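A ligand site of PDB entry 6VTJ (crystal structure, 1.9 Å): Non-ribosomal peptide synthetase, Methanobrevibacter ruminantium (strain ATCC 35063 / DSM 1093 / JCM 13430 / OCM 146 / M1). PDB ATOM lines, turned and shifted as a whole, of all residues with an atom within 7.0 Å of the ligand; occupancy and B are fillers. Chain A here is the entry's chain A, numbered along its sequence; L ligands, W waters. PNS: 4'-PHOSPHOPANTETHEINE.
The backbone NH of Leu 340 is in hydrogen-bond range of the side-chain amide oxygen of Asn 337 (2.9 Å). O of Asn 337 lies within hydrogen-bond range of ND2 of Asn 341 (3.1 Å). The backbone carbonyl oxygen of Ser 46 lies within hydrogen-bond range of the side-chain hydroxyl of Tyr 65. The side-chain amide oxygen (OD1) of Asn 337 sits at hydrogen-bond distance from the backbone NH (N) of Phe 339 (3.1 Å). NE2 of Gln 331 sits at hydrogen-bond distance from OG1 of Thr 336 (3.3 Å).
Water W2 lies within hydrogen-bond range of O26 of the ligand (2.8 Å), OG of Ser 46 (3.1 Å) and N of Leu 47 (3.3 Å). Water W1 lies within hydrogen-bond range of the backbone NH (N) of Ser 46 and an oxygen (O23) of the ligand.
Residues that only touch the ligand: Leu 47 (3.9 Å), Tyr 65 (3.7 Å), Tyr 224 (3.6 Å) and Asn 337 (3.7 Å). Hydrophobic or aromatic side chains that line the ligand: Leu 47, His 223 and Ala 338. Of the 23 residues printed, 10 come within 4 Å of the ligand. The nearest printed residue that does not touch the ligand is Thr 435 (4.004 Å).
A phosphorus (P24) of the ligand is bonded to the side-chain hydroxyl of Ser 46, 1.5 Å away. N36 of the ligand is in hydrogen-bond range of O of Thr 336 (2.9 Å). N of His 223 is in hydrogen-bond range of O35 of the ligand (2.9 Å). A nitrogen (N41) of the ligand lies close to the backbone carbonyl oxygen of Val 221 (3.5 Å). O40 of the ligand sits at hydrogen-bond distance from N of Ala 338, 3.0 Å away. An oxygen (O23) of the ligand lies within salt-bridge range of the side-chain amino group (NZ) of Lys 222.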
ATOM      1  N   THR A  45     -19.224   4.851 -22.803  1.00  0.00           N
ATOM      2  CA  THR A  45     -20.264   5.816 -23.084  1.00  0.00           C
ATOM      3  C   THR A  45     -20.902   6.276 -21.773  1.00  0.00           C
ATOM      4  O   THR A  45     -20.651   5.723 -20.704  1.00  0.00           O
ATOM      5  CB  THR A  45     -21.348   5.213 -23.985  1.00  0.00           C
ATOM      6  OG1 THR A  45     -21.950   4.096 -23.312  1.00  0.00           O
ATOM      7  CG2 THR A  45     -20.744   4.764 -25.319  1.00  0.00           C
ATOM      8  N   SER A  46     -21.762   7.278 -21.904  1.00  0.00           N
ATOM      9  CA  SER A  46     -22.443   7.840 -20.746  1.00  0.00           C
ATOM     10  C   SER A  46     -23.371   6.813 -20.094  1.00  0.00           C
ATOM     11  O   SER A  46     -23.566   6.853 -18.882  1.00  0.00           O
ATOM     12  CB  SER A  46     -23.222   9.076 -21.159  1.00  0.00           C
ATOM     13  OG  SER A  46     -24.309   8.688 -21.995  1.00  0.00           O
ATOM     14  N   LEU A  47     -23.951   5.897 -20.871  1.00  0.00           N
ATOM     15  CA  LEU A  47     -24.812   4.891 -20.254  1.00  0.00           C
ATOM     16  C   LEU A  47     -24.000   3.733 -19.677  1.00  0.00           C
ATOM     17  O   LEU A  47     -24.428   3.134 -18.685  1.00  0.00           O
ATOM     18  CB  LEU A  47     -25.838   4.389 -21.269  1.00  0.00           C
ATOM     19  CG  LEU A  47     -26.862   5.454 -21.693  1.00  0.00           C
ATOM     20  CD1 LEU A  47     -27.926   4.882 -22.613  1.00  0.00           C
ATOM     21  CD2 LEU A  47     -27.490   6.123 -20.469  1.00  0.00           C
ATOM     22  N   TYR A  65     -22.521   9.450 -10.214  1.00  0.00           N
ATOM     23  CA  TYR A  65     -22.387   9.499 -11.670  1.00  0.00           C
ATOM     24  C   TYR A  65     -21.424  10.593 -12.132  1.00  0.00           C
ATOM     25  O   TYR A  65     -20.635  10.370 -13.053  1.00  0.00           O
ATOM     26  CB  TYR A  65     -23.777   9.715 -12.267  1.00  0.00           C
ATOM     27  CG  TYR A  65     -23.923   9.463 -13.743  1.00  0.00           C
ATOM     28  CD1 TYR A  65     -23.463   8.294 -14.332  1.00  0.00           C
ATOM     29  CD2 TYR A  65     -24.587  10.378 -14.549  1.00  0.00           C
ATOM     30  CE1 TYR A  65     -23.637   8.065 -15.702  1.00  0.00           C
ATOM     31  CE2 TYR A  65     -24.763  10.159 -15.899  1.00  0.00           C
ATOM     32  CZ  TYR A  65     -24.299   9.017 -16.476  1.00  0.00           C
ATOM     33  OH  TYR A  65     -24.485   8.833 -17.833  1.00  0.00           O
ATOM     34  N   PHE A  69     -17.362  11.401 -14.915  1.00  0.00           N
ATOM     35  CA  PHE A  69     -17.153  12.467 -15.883  1.00  0.00           C
ATOM     36  C   PHE A  69     -16.039  13.429 -15.445  1.00  0.00           C
ATOM     37  O   PHE A  69     -15.322  13.959 -16.295  1.00  0.00           O
ATOM     38  CB  PHE A  69     -18.459  13.243 -16.104  1.00  0.00           C
ATOM     39  CG  PHE A  69     -19.475  12.454 -16.868  1.00  0.00           C
ATOM     40  CD1 PHE A  69     -19.492  12.500 -18.259  1.00  0.00           C
ATOM     41  CD2 PHE A  69     -20.385  11.644 -16.206  1.00  0.00           C
ATOM     42  CE1 PHE A  69     -20.417  11.762 -18.977  1.00  0.00           C
ATOM     43  CE2 PHE A  69     -21.303  10.894 -16.921  1.00  0.00           C
ATOM     44  CZ  PHE A  69     -21.321  10.964 -18.310  1.00  0.00           C
ATOM     45  N   VAL A 221     -29.114  18.969 -24.493  1.00  0.00           N
ATOM     46  CA  VAL A 221     -29.625  18.961 -23.122  1.00  0.00           C
ATOM     47  C   VAL A 221     -29.143  17.727 -22.360  1.00  0.00           C
ATOM     48  O   VAL A 221     -29.874  17.179 -21.532  1.00  0.00           O
ATOM     49  CB  VAL A 221     -31.174  19.068 -23.095  1.00  0.00           C
ATOM     50  CG1 VAL A 221     -31.629  20.269 -23.914  1.00  0.00           C
ATOM     51  CG2 VAL A 221     -31.875  17.816 -23.617  1.00  0.00           C
ATOM     52  N   LYS A 222     -27.892  17.326 -22.572  1.00  0.00           N
ATOM     53  CA  LYS A 222     -27.293  16.306 -21.715  1.00  0.00           C
ATOM     54  C   LYS A 222     -26.776  16.934 -20.418  1.00  0.00           C
ATOM     55  O   LYS A 222     -26.060  17.945 -20.455  1.00  0.00           O
ATOM     56  CB  LYS A 222     -26.153  15.597 -22.469  1.00  0.00           C
ATOM     57  CG  LYS A 222     -26.670  14.699 -23.584  1.00  0.00           C
ATOM     58  CD  LYS A 222     -25.585  13.905 -24.286  1.00  0.00           C
ATOM     59  CE  LYS A 222     -26.243  12.763 -25.034  1.00  0.00           C
ATOM     60  NZ  LYS A 222     -25.281  12.008 -25.879  1.00  0.00           N
ATOM     61  N   HIS A 223     -27.136  16.349 -19.278  1.00  0.00           N
ATOM     62  CA  HIS A 223     -26.704  16.893 -17.996  1.00  0.00           C
ATOM     63  C   HIS A 223     -25.249  16.561 -17.681  1.00  0.00           C
ATOM     64  O   HIS A 223     -24.653  17.238 -16.841  1.00  0.00           O
ATOM     65  CB  HIS A 223     -27.587  16.367 -16.852  1.00  0.00           C
ATOM     66  N   TYR A 224     -24.683  15.527 -18.303  1.00  0.00           N
ATOM     67  CA  TYR A 224     -23.294  15.125 -18.084  1.00  0.00           C
ATOM     68  C   TYR A 224     -22.703  14.702 -19.421  1.00  0.00           C
ATOM     69  O   TYR A 224     -23.258  13.835 -20.100  1.00  0.00           O
ATOM     70  CB  TYR A 224     -23.200  13.979 -17.066  1.00  0.00           C
ATOM     71  CG  TYR A 224     -23.897  14.319 -15.782  1.00  0.00           C
ATOM     72  CD1 TYR A 224     -23.279  15.110 -14.831  1.00  0.00           C
ATOM     73  CD2 TYR A 224     -25.203  13.887 -15.526  1.00  0.00           C
ATOM     74  CE1 TYR A 224     -23.907  15.453 -13.667  1.00  0.00           C
ATOM     75  CE2 TYR A 224     -25.838  14.228 -14.347  1.00  0.00           C
ATOM     76  CZ  TYR A 224     -25.183  15.018 -13.422  1.00  0.00           C
ATOM     77  OH  TYR A 224     -25.794  15.363 -12.243  1.00  0.00           O
ATOM     78  N   THR A 225     -21.595  15.322 -19.795  1.00  0.00           N
ATOM     79  CA  THR A 225     -20.900  14.972 -21.030  1.00  0.00           C
ATOM     80  C   THR A 225     -19.405  14.971 -20.764  1.00  0.00           C
ATOM     81  O   THR A 225     -18.914  15.653 -19.860  1.00  0.00           O
ATOM     82  CB  THR A 225     -21.182  15.951 -22.185  1.00  0.00           C
ATOM     83  OG1 THR A 225     -20.242  17.031 -22.124  1.00  0.00           O
ATOM     84  CG2 THR A 225     -22.595  16.524 -22.101  1.00  0.00           C
ATOM     85  N   ALA A 226     -18.687  14.210 -21.586  1.00  0.00           N
ATOM     86  CA  ALA A 226     -17.250  14.062 -21.428  1.00  0.00           C
ATOM     87  C   ALA A 226     -16.427  15.095 -22.186  1.00  0.00           C
ATOM     88  O   ALA A 226     -15.225  15.190 -21.956  1.00  0.00           O
ATOM     89  CB  ALA A 226     -16.804  12.660 -21.864  1.00  0.00           C
ATOM     90  N   TYR A 292     -24.200  21.581 -18.180  1.00  0.00           N
ATOM     91  CA  TYR A 292     -25.370  22.031 -18.914  1.00  0.00           C
ATOM     92  C   TYR A 292     -25.927  23.306 -18.309  1.00  0.00           C
ATOM     93  O   TYR A 292     -26.210  24.270 -19.029  1.00  0.00           O
ATOM     94  CB  TYR A 292     -26.418  20.928 -18.923  1.00  0.00           C
ATOM     95  CG  TYR A 292     -27.758  21.434 -19.379  1.00  0.00           C
ATOM     96  CD1 TYR A 292     -27.979  21.728 -20.714  1.00  0.00           C
ATOM     97  CD2 TYR A 292     -28.797  21.634 -18.473  1.00  0.00           C
ATOM     98  CE1 TYR A 292     -29.202  22.201 -21.139  1.00  0.00           C
ATOM     99  CE2 TYR A 292     -30.015  22.110 -18.889  1.00  0.00           C
ATOM    100  CZ  TYR A 292     -30.201  22.389 -20.233  1.00  0.00           C
ATOM    101  OH  TYR A 292     -31.403  22.863 -20.667  1.00  0.00           O
ATOM    102  N   ASN A 320     -39.633  21.319 -16.614  1.00  0.00           N
ATOM    103  CA  ASN A 320     -39.691  19.867 -16.847  1.00  0.00           C
ATOM    104  C   ASN A 320     -40.586  19.612 -18.057  1.00  0.00           C
ATOM    105  O   ASN A 320     -41.815  19.487 -17.926  1.00  0.00           O
ATOM    106  CB  ASN A 320     -40.186  19.176 -15.581  1.00  0.00           C
ATOM    107  CG  ASN A 320     -40.274  17.651 -15.720  1.00  0.00           C
ATOM    108  OD1 ASN A 320     -39.493  17.015 -16.429  1.00  0.00           O
ATOM    109  ND2 ASN A 320     -41.221  17.060 -15.003  1.00  0.00           N
ATOM    110  N   GLN A 331     -41.413  12.767 -26.466  1.00  0.00           N
ATOM    111  CA  GLN A 331     -40.406  12.971 -27.508  1.00  0.00           C
ATOM    112  C   GLN A 331     -40.065  11.648 -28.211  1.00  0.00           C
ATOM    113  O   GLN A 331     -40.281  10.553 -27.683  1.00  0.00           O
ATOM    114  CB  GLN A 331     -39.143  13.613 -26.921  1.00  0.00           C
ATOM    115  CG  GLN A 331     -38.330  12.728 -26.028  1.00  0.00           C
ATOM    116  CD  GLN A 331     -37.498  13.520 -25.031  1.00  0.00           C
ATOM    117  OE1 GLN A 331     -37.775  14.684 -24.754  1.00  0.00           O
ATOM    118  NE2 GLN A 331     -36.482  12.875 -24.473  1.00  0.00           N
ATOM    119  N   ASP A 335     -36.447   7.588 -24.231  1.00  0.00           N
ATOM    120  CA  ASP A 335     -35.664   6.807 -23.281  1.00  0.00           C
ATOM    121  C   ASP A 335     -34.652   7.636 -22.507  1.00  0.00           C
ATOM    122  O   ASP A 335     -34.113   7.145 -21.509  1.00  0.00           O
ATOM    123  CB  ASP A 335     -34.942   5.679 -24.004  1.00  0.00           C
ATOM    124  CG  ASP A 335     -35.873   4.589 -24.474  1.00  0.00           C
ATOM    125  OD1 ASP A 335     -37.033   4.550 -24.015  1.00  0.00           O
ATOM    126  OD2 ASP A 335     -35.458   3.761 -25.319  1.00  0.00           O
ATOM    127  N   THR A 336     -34.397   8.877 -22.918  1.00  0.00           N
ATOM    128  CA  THR A 336     -33.285   9.681 -22.403  1.00  0.00           C
ATOM    129  C   THR A 336     -33.668  10.712 -21.346  1.00  0.00           C
ATOM    130  O   THR A 336     -32.789  11.443 -20.869  1.00  0.00           O
ATOM    131  CB  THR A 336     -32.617  10.400 -23.569  1.00  0.00           C
ATOM    132  OG1 THR A 336     -33.556  11.329 -24.130  1.00  0.00           O
ATOM    133  CG2 THR A 336     -32.217   9.391 -24.641  1.00  0.00           C
ATOM    134  N   ASN A 337     -34.952  10.813 -20.985  1.00  0.00           N
ATOM    135  CA  ASN A 337     -35.396  11.816 -20.029  1.00  0.00           C
ATOM    136  C   ASN A 337     -35.067  11.398 -18.595  1.00  0.00           C
ATOM    137  O   ASN A 337     -35.464  10.311 -18.166  1.00  0.00           O
ATOM    138  CB  ASN A 337     -36.903  12.037 -20.149  1.00  0.00           C
ATOM    139  CG  ASN A 337     -37.363  13.203 -19.344  1.00  0.00           C
ATOM    140  OD1 ASN A 337     -37.794  13.045 -18.194  1.00  0.00           O
ATOM    141  ND2 ASN A 337     -37.247  14.409 -19.924  1.00  0.00           N
ATOM    142  N   ALA A 338     -34.413  12.292 -17.842  1.00  0.00           N
ATOM    143  CA  ALA A 338     -33.976  11.941 -16.487  1.00  0.00           C
ATOM    144  C   ALA A 338     -35.136  11.854 -15.490  1.00  0.00           C
ATOM    145  O   ALA A 338     -35.161  10.952 -14.641  1.00  0.00           O
ATOM    146  CB  ALA A 338     -32.928  12.950 -15.992  1.00  0.00           C
ATOM    147  N   PHE A 339     -36.094  12.776 -15.564  1.00  0.00           N
ATOM    148  CA  PHE A 339     -37.252  12.707 -14.675  1.00  0.00           C
ATOM    149  C   PHE A 339     -38.014  11.396 -14.869  1.00  0.00           C
ATOM    150  O   PHE A 339     -38.362  10.714 -13.905  1.00  0.00           O
ATOM    151  CB  PHE A 339     -38.160  13.921 -14.948  1.00  0.00           C
ATOM    152  CG  PHE A 339     -39.524  13.838 -14.299  1.00  0.00           C
ATOM    153  CD1 PHE A 339     -39.684  14.087 -12.956  1.00  0.00           C
ATOM    154  CD2 PHE A 339     -40.636  13.526 -15.060  1.00  0.00           C
ATOM    155  CE1 PHE A 339     -40.941  14.008 -12.375  1.00  0.00           C
ATOM    156  CE2 PHE A 339     -41.878  13.455 -14.476  1.00  0.00           C
ATOM    157  CZ  PHE A 339     -42.023  13.712 -13.131  1.00  0.00           C
ATOM    158  N   LEU A 340     -38.264  11.026 -16.126  1.00  0.00           N
ATOM    159  CA  LEU A 340     -38.996   9.787 -16.368  1.00  0.00           C
ATOM    160  C   LEU A 340     -38.165   8.564 -15.992  1.00  0.00           C
ATOM    161  O   LEU A 340     -38.716   7.588 -15.524  1.00  0.00           O
ATOM    162  CB  LEU A 340     -39.456   9.707 -17.828  1.00  0.00           C
ATOM    163  CG  LEU A 340     -40.596  10.674 -18.194  1.00  0.00           C
ATOM    164  CD1 LEU A 340     -40.826  10.704 -19.685  1.00  0.00           C
ATOM    165  CD2 LEU A 340     -41.885  10.347 -17.504  1.00  0.00           C
ATOM    166  N   ASN A 341     -36.840   8.585 -16.185  1.00  0.00           N
ATOM    167  CA  ASN A 341     -36.058   7.408 -15.816  1.00  0.00           C
ATOM    168  C   ASN A 341     -35.989   7.229 -14.309  1.00  0.00           C
ATOM    169  O   ASN A 341     -35.923   6.103 -13.808  1.00  0.00           O
ATOM    170  CB  ASN A 341     -34.629   7.500 -16.404  1.00  0.00           C
ATOM    171  CG  ASN A 341     -34.585   7.175 -17.888  1.00  0.00           C
ATOM    172  OD1 ASN A 341     -35.388   6.382 -18.399  1.00  0.00           O
ATOM    173  ND2 ASN A 341     -33.664   7.801 -18.595  1.00  0.00           N
ATOM    174  N   THR A 435     -28.173   7.658 -13.154  1.00  0.00           N
ATOM    175  CA  THR A 435     -27.758   8.629 -14.164  1.00  0.00           C
ATOM    176  C   THR A 435     -28.253  10.027 -13.820  1.00  0.00           C
ATOM    177  O   THR A 435     -27.829  10.996 -14.459  1.00  0.00           O
ATOM    178  CB  THR A 435     -28.255   8.251 -15.577  1.00  0.00           C
ATOM    179  OG1 THR A 435     -29.677   8.162 -15.593  1.00  0.00           O
ATOM    180  CG2 THR A 435     -27.648   6.925 -16.037  1.00  0.00           C
ATOM    181  N   ALA A 436     -29.111  10.139 -12.811  1.00  0.00           N
ATOM    182  CA  ALA A 436     -29.536  11.396 -12.232  1.00  0.00           C
ATOM    183  C   ALA A 436     -28.654  11.844 -11.082  1.00  0.00           C
ATOM    184  O   ALA A 436     -29.070  12.704 -10.293  1.00  0.00           O
ATOM    185  CB  ALA A 436     -30.993  11.297 -11.777  1.00  0.00           C
HETATM  186  O23 PNS L   1     -24.150  10.564 -23.614  1.00  0.00           O
HETATM  187  P24 PNS L   1     -24.982   9.582 -22.926  1.00  0.00           P
HETATM  188  O26 PNS L   1     -25.888   8.810 -23.730  1.00  0.00           O
HETATM  189  O27 PNS L   1     -25.922  10.429 -22.064  1.00  0.00           O
HETATM  190  C28 PNS L   1     -26.650   9.891 -20.991  1.00  0.00           C
HETATM  191  C29 PNS L   1     -27.234  10.962 -20.080  1.00  0.00           C
HETATM  192  C30 PNS L   1     -28.056  10.270 -19.029  1.00  0.00           C
HETATM  193  C31 PNS L   1     -26.112  11.706 -19.390  1.00  0.00           C
HETATM  194  C32 PNS L   1     -28.148  11.885 -20.909  1.00  0.00           C
HETATM  195  O33 PNS L   1     -28.975  11.088 -21.715  1.00  0.00           O
HETATM  196  C34 PNS L   1     -28.954  12.845 -20.061  1.00  0.00           C
HETATM  197  O35 PNS L   1     -28.373  13.683 -19.451  1.00  0.00           O
HETATM  198  N36 PNS L   1     -30.288  12.731 -20.049  1.00  0.00           N
HETATM  199  C37 PNS L   1     -31.189  13.592 -19.355  1.00  0.00           C
HETATM  200  C38 PNS L   1     -31.625  14.797 -20.149  1.00  0.00           C
HETATM  201  C39 PNS L   1     -32.774  15.510 -19.517  1.00  0.00           C
HETATM  202  O40 PNS L   1     -33.668  14.917 -19.015  1.00  0.00           O
HETATM  203  N41 PNS L   1     -32.730  16.797 -19.574  1.00  0.00           N
HETATM  204  O   HOH W   1     -21.580   8.862 -24.261  1.00  0.00           O
HETATM  205  O   HOH W   2     -24.772   6.301 -23.990  1.00  0.00           O
